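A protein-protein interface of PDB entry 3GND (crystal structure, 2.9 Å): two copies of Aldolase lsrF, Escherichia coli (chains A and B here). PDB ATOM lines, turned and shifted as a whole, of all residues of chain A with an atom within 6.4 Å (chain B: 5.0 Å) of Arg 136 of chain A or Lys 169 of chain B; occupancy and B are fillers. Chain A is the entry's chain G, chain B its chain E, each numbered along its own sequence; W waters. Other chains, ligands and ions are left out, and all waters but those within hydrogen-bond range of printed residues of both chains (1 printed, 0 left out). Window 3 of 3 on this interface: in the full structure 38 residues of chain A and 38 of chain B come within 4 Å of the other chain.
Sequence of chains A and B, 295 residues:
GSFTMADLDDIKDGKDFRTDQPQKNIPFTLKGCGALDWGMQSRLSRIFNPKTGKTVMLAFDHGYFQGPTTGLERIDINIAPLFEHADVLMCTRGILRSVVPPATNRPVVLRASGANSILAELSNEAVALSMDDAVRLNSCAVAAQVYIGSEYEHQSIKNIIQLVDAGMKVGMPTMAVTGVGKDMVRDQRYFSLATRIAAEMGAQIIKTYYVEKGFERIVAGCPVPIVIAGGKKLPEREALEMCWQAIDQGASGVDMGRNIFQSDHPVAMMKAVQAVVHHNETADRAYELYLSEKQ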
ATOM      1  N   ARG A  97       2.959 -15.924   5.306  1.00  0.00           N
ATOM      2  CA  ARG A  97       2.670 -15.994   3.881  1.00  0.00           C
ATOM      3  C   ARG A  97       3.066 -17.321   3.245  1.00  0.00           C
ATOM      4  O   ARG A  97       2.332 -17.873   2.415  1.00  0.00           O
ATOM      5  CB  ARG A  97       3.346 -14.867   3.151  1.00  0.00           C
ATOM      6  CG  ARG A  97       2.662 -13.558   3.370  1.00  0.00           C
ATOM      7  CD  ARG A  97       3.116 -12.508   2.375  1.00  0.00           C
ATOM      8  NE  ARG A  97       3.221 -11.192   2.997  1.00  0.00           N
ATOM      9  CZ  ARG A  97       2.319 -10.224   2.852  1.00  0.00           C
ATOM     10  NH1 ARG A  97       1.255 -10.423   2.097  1.00  0.00           N
ATOM     11  NH2 ARG A  97       2.481  -9.051   3.447  1.00  0.00           N
ATOM     12  N   SER A 130       6.135  -2.992   8.679  1.00  0.00           N
ATOM     13  CA  SER A 130       5.317  -1.773   8.763  1.00  0.00           C
ATOM     14  C   SER A 130       3.852  -2.086   9.106  1.00  0.00           C
ATOM     15  O   SER A 130       3.324  -3.171   8.743  1.00  0.00           O
ATOM     16  CB  SER A 130       5.331  -1.063   7.425  1.00  0.00           C
ATOM     17  OG  SER A 130       4.646  -1.825   6.441  1.00  0.00           O
ATOM     18  N   MET A 131       3.187  -1.130   9.768  1.00  0.00           N
ATOM     19  CA  MET A 131       1.810  -1.291  10.204  1.00  0.00           C
ATOM     20  C   MET A 131       0.992  -1.497   8.922  1.00  0.00           C
ATOM     21  O   MET A 131       0.030  -2.314   8.870  1.00  0.00           O
ATOM     22  CB  MET A 131       1.350  -0.047  10.965  1.00  0.00           C
ATOM     23  CG  MET A 131      -0.052  -0.165  11.503  1.00  0.00           C
ATOM     24  SD  MET A 131      -0.263  -1.638  12.534  1.00  0.00           S
ATOM     25  CE  MET A 131       0.744  -1.176  13.977  1.00  0.00           C
ATOM     26  N   ASP A 132       1.397  -0.761   7.880  1.00  0.00           N
ATOM     27  CA  ASP A 132       0.866  -0.968   6.527  1.00  0.00           C
ATOM     28  C   ASP A 132       0.630  -2.476   6.183  1.00  0.00           C
ATOM     29  O   ASP A 132      -0.478  -2.910   5.817  1.00  0.00           O
ATOM     30  CB  ASP A 132       1.833  -0.353   5.530  1.00  0.00           C
ATOM     31  CG  ASP A 132       1.344  -0.455   4.125  1.00  0.00           C
ATOM     32  OD1 ASP A 132       0.257   0.061   3.837  1.00  0.00           O
ATOM     33  OD2 ASP A 132       2.051  -1.030   3.291  1.00  0.00           O
ATOM     34  N   ASP A 133       1.701  -3.257   6.313  1.00  0.00           N
ATOM     35  CA  ASP A 133       1.665  -4.643   5.943  1.00  0.00           C
ATOM     36  C   ASP A 133       0.929  -5.461   6.978  1.00  0.00           C
ATOM     37  O   ASP A 133       0.424  -6.549   6.647  1.00  0.00           O
ATOM     38  CB  ASP A 133       3.085  -5.187   5.763  1.00  0.00           C
ATOM     39  CG  ASP A 133       3.121  -6.371   4.797  1.00  0.00           C
ATOM     40  OD1 ASP A 133       2.272  -6.375   3.862  1.00  0.00           O
ATOM     41  OD2 ASP A 133       3.982  -7.288   4.961  1.00  0.00           O
ATOM     42  N   ALA A 134       0.896  -4.974   8.228  1.00  0.00           N
ATOM     43  CA  ALA A 134       0.180  -5.703   9.279  1.00  0.00           C
ATOM     44  C   ALA A 134      -1.291  -5.668   8.921  1.00  0.00           C
ATOM     45  O   ALA A 134      -2.000  -6.686   9.002  1.00  0.00           O
ATOM     46  CB  ALA A 134       0.389  -5.106  10.657  1.00  0.00           C
ATOM     47  N   VAL A 135      -1.747  -4.502   8.487  1.00  0.00           N
ATOM     48  CA  VAL A 135      -3.147  -4.363   8.125  1.00  0.00           C
ATOM     49  C   VAL A 135      -3.434  -5.172   6.859  1.00  0.00           C
ATOM     50  O   VAL A 135      -4.516  -5.784   6.742  1.00  0.00           O
ATOM     51  CB  VAL A 135      -3.554  -2.893   7.962  1.00  0.00           C
ATOM     52  CG1 VAL A 135      -4.866  -2.769   7.212  1.00  0.00           C
ATOM     53  CG2 VAL A 135      -3.643  -2.260   9.301  1.00  0.00           C
ATOM     54  N   ARG A 136      -2.464  -5.211   5.939  1.00  0.00           N
ATOM     55  CA  ARG A 136      -2.639  -5.967   4.691  1.00  0.00           C
ATOM     56  C   ARG A 136      -2.817  -7.435   5.035  1.00  0.00           C
ATOM     57  O   ARG A 136      -3.617  -8.157   4.389  1.00  0.00           O
ATOM     58  CB  ARG A 136      -1.455  -5.809   3.761  1.00  0.00           C
ATOM     59  CG  ARG A 136      -1.681  -6.386   2.393  1.00  0.00           C
ATOM     60  CD  ARG A 136      -0.453  -6.176   1.484  1.00  0.00           C
ATOM     61  NE  ARG A 136      -0.288  -4.759   1.099  1.00  0.00           N
ATOM     62  CZ  ARG A 136       0.487  -3.883   1.730  1.00  0.00           C
ATOM     63  NH1 ARG A 136       1.204  -4.227   2.796  1.00  0.00           N
ATOM     64  NH2 ARG A 136       0.520  -2.651   1.282  1.00  0.00           N
ATOM     65  N   LEU A 137      -2.087  -7.878   6.059  1.00  0.00           N
ATOM     66  CA  LEU A 137      -2.161  -9.268   6.477  1.00  0.00           C
ATOM     67  C   LEU A 137      -3.355  -9.595   7.386  1.00  0.00           C
ATOM     68  O   LEU A 137      -3.498 -10.769   7.831  1.00  0.00           O
ATOM     69  CB  LEU A 137      -0.878  -9.706   7.153  1.00  0.00           C
ATOM     70  CG  LEU A 137       0.230  -9.915   6.139  1.00  0.00           C
ATOM     71  CD1 LEU A 137       1.593 -10.051   6.852  1.00  0.00           C
ATOM     72  CD2 LEU A 137      -0.045 -11.146   5.283  1.00  0.00           C
ATOM     73  N   ASN A 138      -4.207  -8.595   7.666  1.00  0.00           N
ATOM     74  CA  ASN A 138      -5.382  -8.819   8.524  1.00  0.00           C
ATOM     75  C   ASN A 138      -5.023  -9.248   9.952  1.00  0.00           C
ATOM     76  O   ASN A 138      -5.714 -10.104  10.509  1.00  0.00           O
ATOM     77  CB  ASN A 138      -6.294  -9.884   7.911  1.00  0.00           C
ATOM     78  CG  ASN A 138      -7.663  -9.902   8.537  1.00  0.00           C
ATOM     79  OD1 ASN A 138      -8.122  -8.874   9.043  1.00  0.00           O
ATOM     80  ND2 ASN A 138      -8.348 -11.073   8.499  1.00  0.00           N
ATOM     81  N   SER A 139      -3.962  -8.681  10.539  1.00  0.00           N
ATOM     82  CA  SER A 139      -3.556  -9.053  11.885  1.00  0.00           C
ATOM     83  C   SER A 139      -4.558  -8.662  12.947  1.00  0.00           C
ATOM     84  O   SER A 139      -5.280  -7.719  12.765  1.00  0.00           O
ATOM     85  CB  SER A 139      -2.283  -8.346  12.249  1.00  0.00           C
ATOM     86  OG  SER A 139      -1.251  -8.720  11.397  1.00  0.00           O
ATOM     87  N   ASP B  37      -3.463 -11.956  -2.181  1.00  0.00           N
ATOM     88  CA  ASP B  37      -2.559 -11.941  -1.045  1.00  0.00           C
ATOM     89  C   ASP B  37      -3.132 -12.599   0.224  1.00  0.00           C
ATOM     90  O   ASP B  37      -4.364 -12.758   0.396  1.00  0.00           O
ATOM     91  CB  ASP B  37      -2.216 -10.497  -0.711  1.00  0.00           C
ATOM     92  CG  ASP B  37      -1.097 -10.397   0.257  1.00  0.00           C
ATOM     93  OD1 ASP B  37      -0.031 -10.963  -0.049  1.00  0.00           O
ATOM     94  OD2 ASP B  37      -1.285  -9.762   1.308  1.00  0.00           O
ATOM     95  N   GLY B  39      -3.554 -11.729   3.371  1.00  0.00           N
ATOM     96  CA  GLY B  39      -4.497 -11.028   4.206  1.00  0.00           C
ATOM     97  C   GLY B  39      -5.871 -11.024   3.563  1.00  0.00           C
ATOM     98  O   GLY B  39      -6.886 -11.136   4.254  1.00  0.00           O
ATOM     99  N   MET B  40      -5.930 -10.873   2.246  1.00  0.00           N
ATOM    100  CA  MET B  40      -7.227 -10.757   1.618  1.00  0.00           C
ATOM    101  C   MET B  40      -7.931 -12.121   1.606  1.00  0.00           C
ATOM    102  O   MET B  40      -9.155 -12.228   1.760  1.00  0.00           O
ATOM    103  CB  MET B  40      -7.109 -10.172   0.201  1.00  0.00           C
ATOM    104  CG  MET B  40      -8.466  -9.924  -0.447  1.00  0.00           C
ATOM    105  SD  MET B  40      -8.417  -8.968  -1.967  1.00  0.00           S
ATOM    106  CE  MET B  40      -8.388  -7.309  -1.311  1.00  0.00           C
ATOM    107  N   ARG B  43      -9.377 -12.604   5.114  1.00  0.00           N
ATOM    108  CA  ARG B  43     -10.648 -11.946   5.318  1.00  0.00           C
ATOM    109  C   ARG B  43     -11.750 -12.708   4.631  1.00  0.00           C
ATOM    110  O   ARG B  43     -12.818 -12.889   5.206  1.00  0.00           O
ATOM    111  CB  ARG B  43     -10.621 -10.494   4.842  1.00  0.00           C
ATOM    112  CG  ARG B  43      -9.704  -9.595   5.662  1.00  0.00           C
ATOM    113  CD  ARG B  43      -9.813  -8.147   5.269  1.00  0.00           C
ATOM    114  NE  ARG B  43      -9.155  -7.318   6.267  1.00  0.00           N
ATOM    115  CZ  ARG B  43      -7.927  -6.806   6.144  1.00  0.00           C
ATOM    116  NH1 ARG B  43      -7.208  -7.033   5.048  1.00  0.00           N
ATOM    117  NH2 ARG B  43      -7.409  -6.047   7.113  1.00  0.00           N
ATOM    118  N   ASP B 165      -9.921   0.102  -5.762  1.00  0.00           N
ATOM    119  CA  ASP B 165      -8.636   0.834  -5.649  1.00  0.00           C
ATOM    120  C   ASP B 165      -8.175   0.943  -4.215  1.00  0.00           C
ATOM    121  O   ASP B 165      -7.041   0.604  -3.914  1.00  0.00           O
ATOM    122  CB  ASP B 165      -8.709   2.254  -6.215  1.00  0.00           C
ATOM    123  CG  ASP B 165      -8.744   2.293  -7.740  1.00  0.00           C
ATOM    124  OD1 ASP B 165      -8.348   1.297  -8.386  1.00  0.00           O
ATOM    125  OD2 ASP B 165      -9.174   3.324  -8.291  1.00  0.00           O
ATOM    126  N   ALA B 166      -9.042   1.412  -3.332  1.00  0.00           N
ATOM    127  CA  ALA B 166      -8.633   1.569  -1.954  1.00  0.00           C
ATOM    128  C   ALA B 166      -8.406   0.232  -1.236  1.00  0.00           C
ATOM    129  O   ALA B 166      -7.467   0.121  -0.447  1.00  0.00           O
ATOM    130  CB  ALA B 166      -9.624   2.393  -1.205  1.00  0.00           C
ATOM    131  N   GLY B 167      -9.267  -0.764  -1.478  1.00  0.00           N
ATOM    132  CA  GLY B 167      -9.163  -2.047  -0.807  1.00  0.00           C
ATOM    133  C   GLY B 167      -7.922  -2.841  -1.185  1.00  0.00           C
ATOM    134  O   GLY B 167      -7.408  -3.639  -0.400  1.00  0.00           O
ATOM    135  N   MET B 168      -7.420  -2.643  -2.394  1.00  0.00           N
ATOM    136  CA  MET B 168      -6.269  -3.400  -2.812  1.00  0.00           C
ATOM    137  C   MET B 168      -5.029  -2.936  -2.095  1.00  0.00           C
ATOM    138  O   MET B 168      -4.125  -3.729  -1.893  1.00  0.00           O
ATOM    139  CB  MET B 168      -6.085  -3.310  -4.311  1.00  0.00           C
ATOM    140  CG  MET B 168      -7.141  -4.074  -5.041  1.00  0.00           C
ATOM    141  SD  MET B 168      -7.263  -5.813  -4.433  1.00  0.00           S
ATOM    142  CE  MET B 168      -8.595  -6.366  -5.474  1.00  0.00           C
ATOM    143  N   LYS B 169      -4.961  -1.665  -1.702  1.00  0.00           N
ATOM    144  CA  LYS B 169      -3.810  -1.195  -0.951  1.00  0.00           C
ATOM    145  C   LYS B 169      -3.723  -1.859   0.432  1.00  0.00           C
ATOM    146  O   LYS B 169      -2.657  -1.901   1.053  1.00  0.00           O
ATOM    147  CB  LYS B 169      -3.873   0.302  -0.742  1.00  0.00           C
ATOM    148  CG  LYS B 169      -3.892   1.161  -1.996  1.00  0.00           C
ATOM    149  CD  LYS B 169      -3.504   2.601  -1.619  1.00  0.00           C
ATOM    150  CE  LYS B 169      -4.133   3.581  -2.552  1.00  0.00           C
ATOM    151  NZ  LYS B 169      -3.337   3.816  -3.759  1.00  0.00           N
ATOM    152  N   VAL B 170      -4.839  -2.393   0.900  1.00  0.00           N
ATOM    153  CA  VAL B 170      -5.003  -2.726   2.294  1.00  0.00           C
ATOM    154  C   VAL B 170      -5.444  -4.187   2.492  1.00  0.00           C
ATOM    155  O   VAL B 170      -5.376  -4.710   3.611  1.00  0.00           O
ATOM    156  CB  VAL B 170      -6.028  -1.773   2.897  1.00  0.00           C
ATOM    157  CG1 VAL B 170      -6.842  -2.471   3.913  1.00  0.00           C
ATOM    158  CG2 VAL B 170      -5.320  -0.604   3.462  1.00  0.00           C
ATOM    159  N   GLY B 171      -5.881  -4.848   1.412  1.00  0.00           N
ATOM    160  CA  GLY B 171      -6.209  -6.274   1.467  1.00  0.00           C
ATOM    161  C   GLY B 171      -7.641  -6.421   1.922  1.00  0.00           C
ATOM    162  O   GLY B 171      -8.001  -7.450   2.492  1.00  0.00           O
HETATM  163  O   HOH W   1      -3.808  -8.701   1.864  1.00  0.00           O
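Among the printed residues, pairs that only touch across the chains: Arg 136 of chain A with Gly 39 of chain B (3.0 Å), Arg 136 of chain A with Val 170 of chain B (3.2 Å), Arg 136 of chain A with Asp 37 of chain B (3.6 Å), Leu 137 of chain A with Gly 39 of chain B (3.7 Å), Arg 136 of chain A with Arg 43 of chain B (3.8 Å) and Asn 138 of chain A with Gly 39 of chain B (3.9 Å).
OD1 of Asp 37 of chain B is in salt-bridge range of NH1 of Arg 97 of chain A, at 2.6 Å. O of Val 135 of chain A is in hydrogen-bond range of NH2 of Arg 43 of chain B (2.9 Å). The side-chain amide oxygen (OD1) of Asn 138 of chain A is in hydrogen-bond range of the guanidinium group (NE) of Arg 43 of chain B. The guanidinium group (NH2) of Arg 136 of chain A is in hydrogen-bond range of the backbone carbonyl oxygen (O) of Lys 169 of chain B. O of Val 135 of chain A lies close to O of Val 170 of chain B, 3.4 Å away.
Water W1 lies within hydrogen-bond range of the backbone carbonyl oxygen of Arg 136 of chain A, the side-chain carboxylate of Asp 37 of chain B, the backbone NH of Met 40 of chain B and the backbone NH of Gly 39 of chain B.
Hydrophobic or aromatic side chains of chain A that line the printed part of chain B: Val 135. Hydrophobic or aromatic side chains of chain B that line the printed part of chain A: Val 170.
No position is printed for both chains.
The guanidinium group (NH1) of Arg 43 of chain B sits at hydrogen-bond distance from the backbone carbonyl oxygen (O) of Val 170 of chain B, at 3.3 Å. O of Gly 171 of chain B lies within hydrogen-bond range of NH1 of Arg 43 of chain B, at 2.7 Å. The guanidinium group (NH2) of Arg 97 of chain A is in salt-bridge range of the side-chain carboxylate (OD1) of Asp 133 of chain A. NH2 of Arg 136 of chain A is in salt-bridge range of OD2 of Asp 132 of chain A, at 3.0 Å. OD1 of Asp 133 of chain A is in salt-bridge range of NH1 of Arg 136 of chain A (2.6 Å).
Of the printed residues of chain B, Arg 97 of chain A touches Asp 37. Ala 134 of chain A touches none of the printed residues of chain B. Of chain B, only Asp 37, Gly 39, Arg 43, Lys 169 and Val 170 come within 4 Å of Arg 136 of chain A. Printed residues of chain B within 4 Å of Asn 138 of chain A: Gly 39 (3.9 Å) and Arg 43 (3.3 Å). Ser 139 of chain A touches none of the printed residues of chain B. Of the printed residues of chain A, Asp 37 of chain B touches Arg 97 and Arg 136. Printed residues of chain A within 4 Å of Gly 39 of chain B: Arg 136, Leu 137 and Asn 138. Printed residues of chain A within 4 Å of Lys 169 of chain B: Arg 136. Printed residues of chain A within 4 Å of Val 170 of chain B: Val 135 and Arg 136. The nearest residue of chain B that does not touch Arg 136 of chain A is Met 40 of chain B (4.2 Å). The nearest printed residue of chain B that does not touch Leu 137 of chain A is Asp 37 of chain B (4.4 Å).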
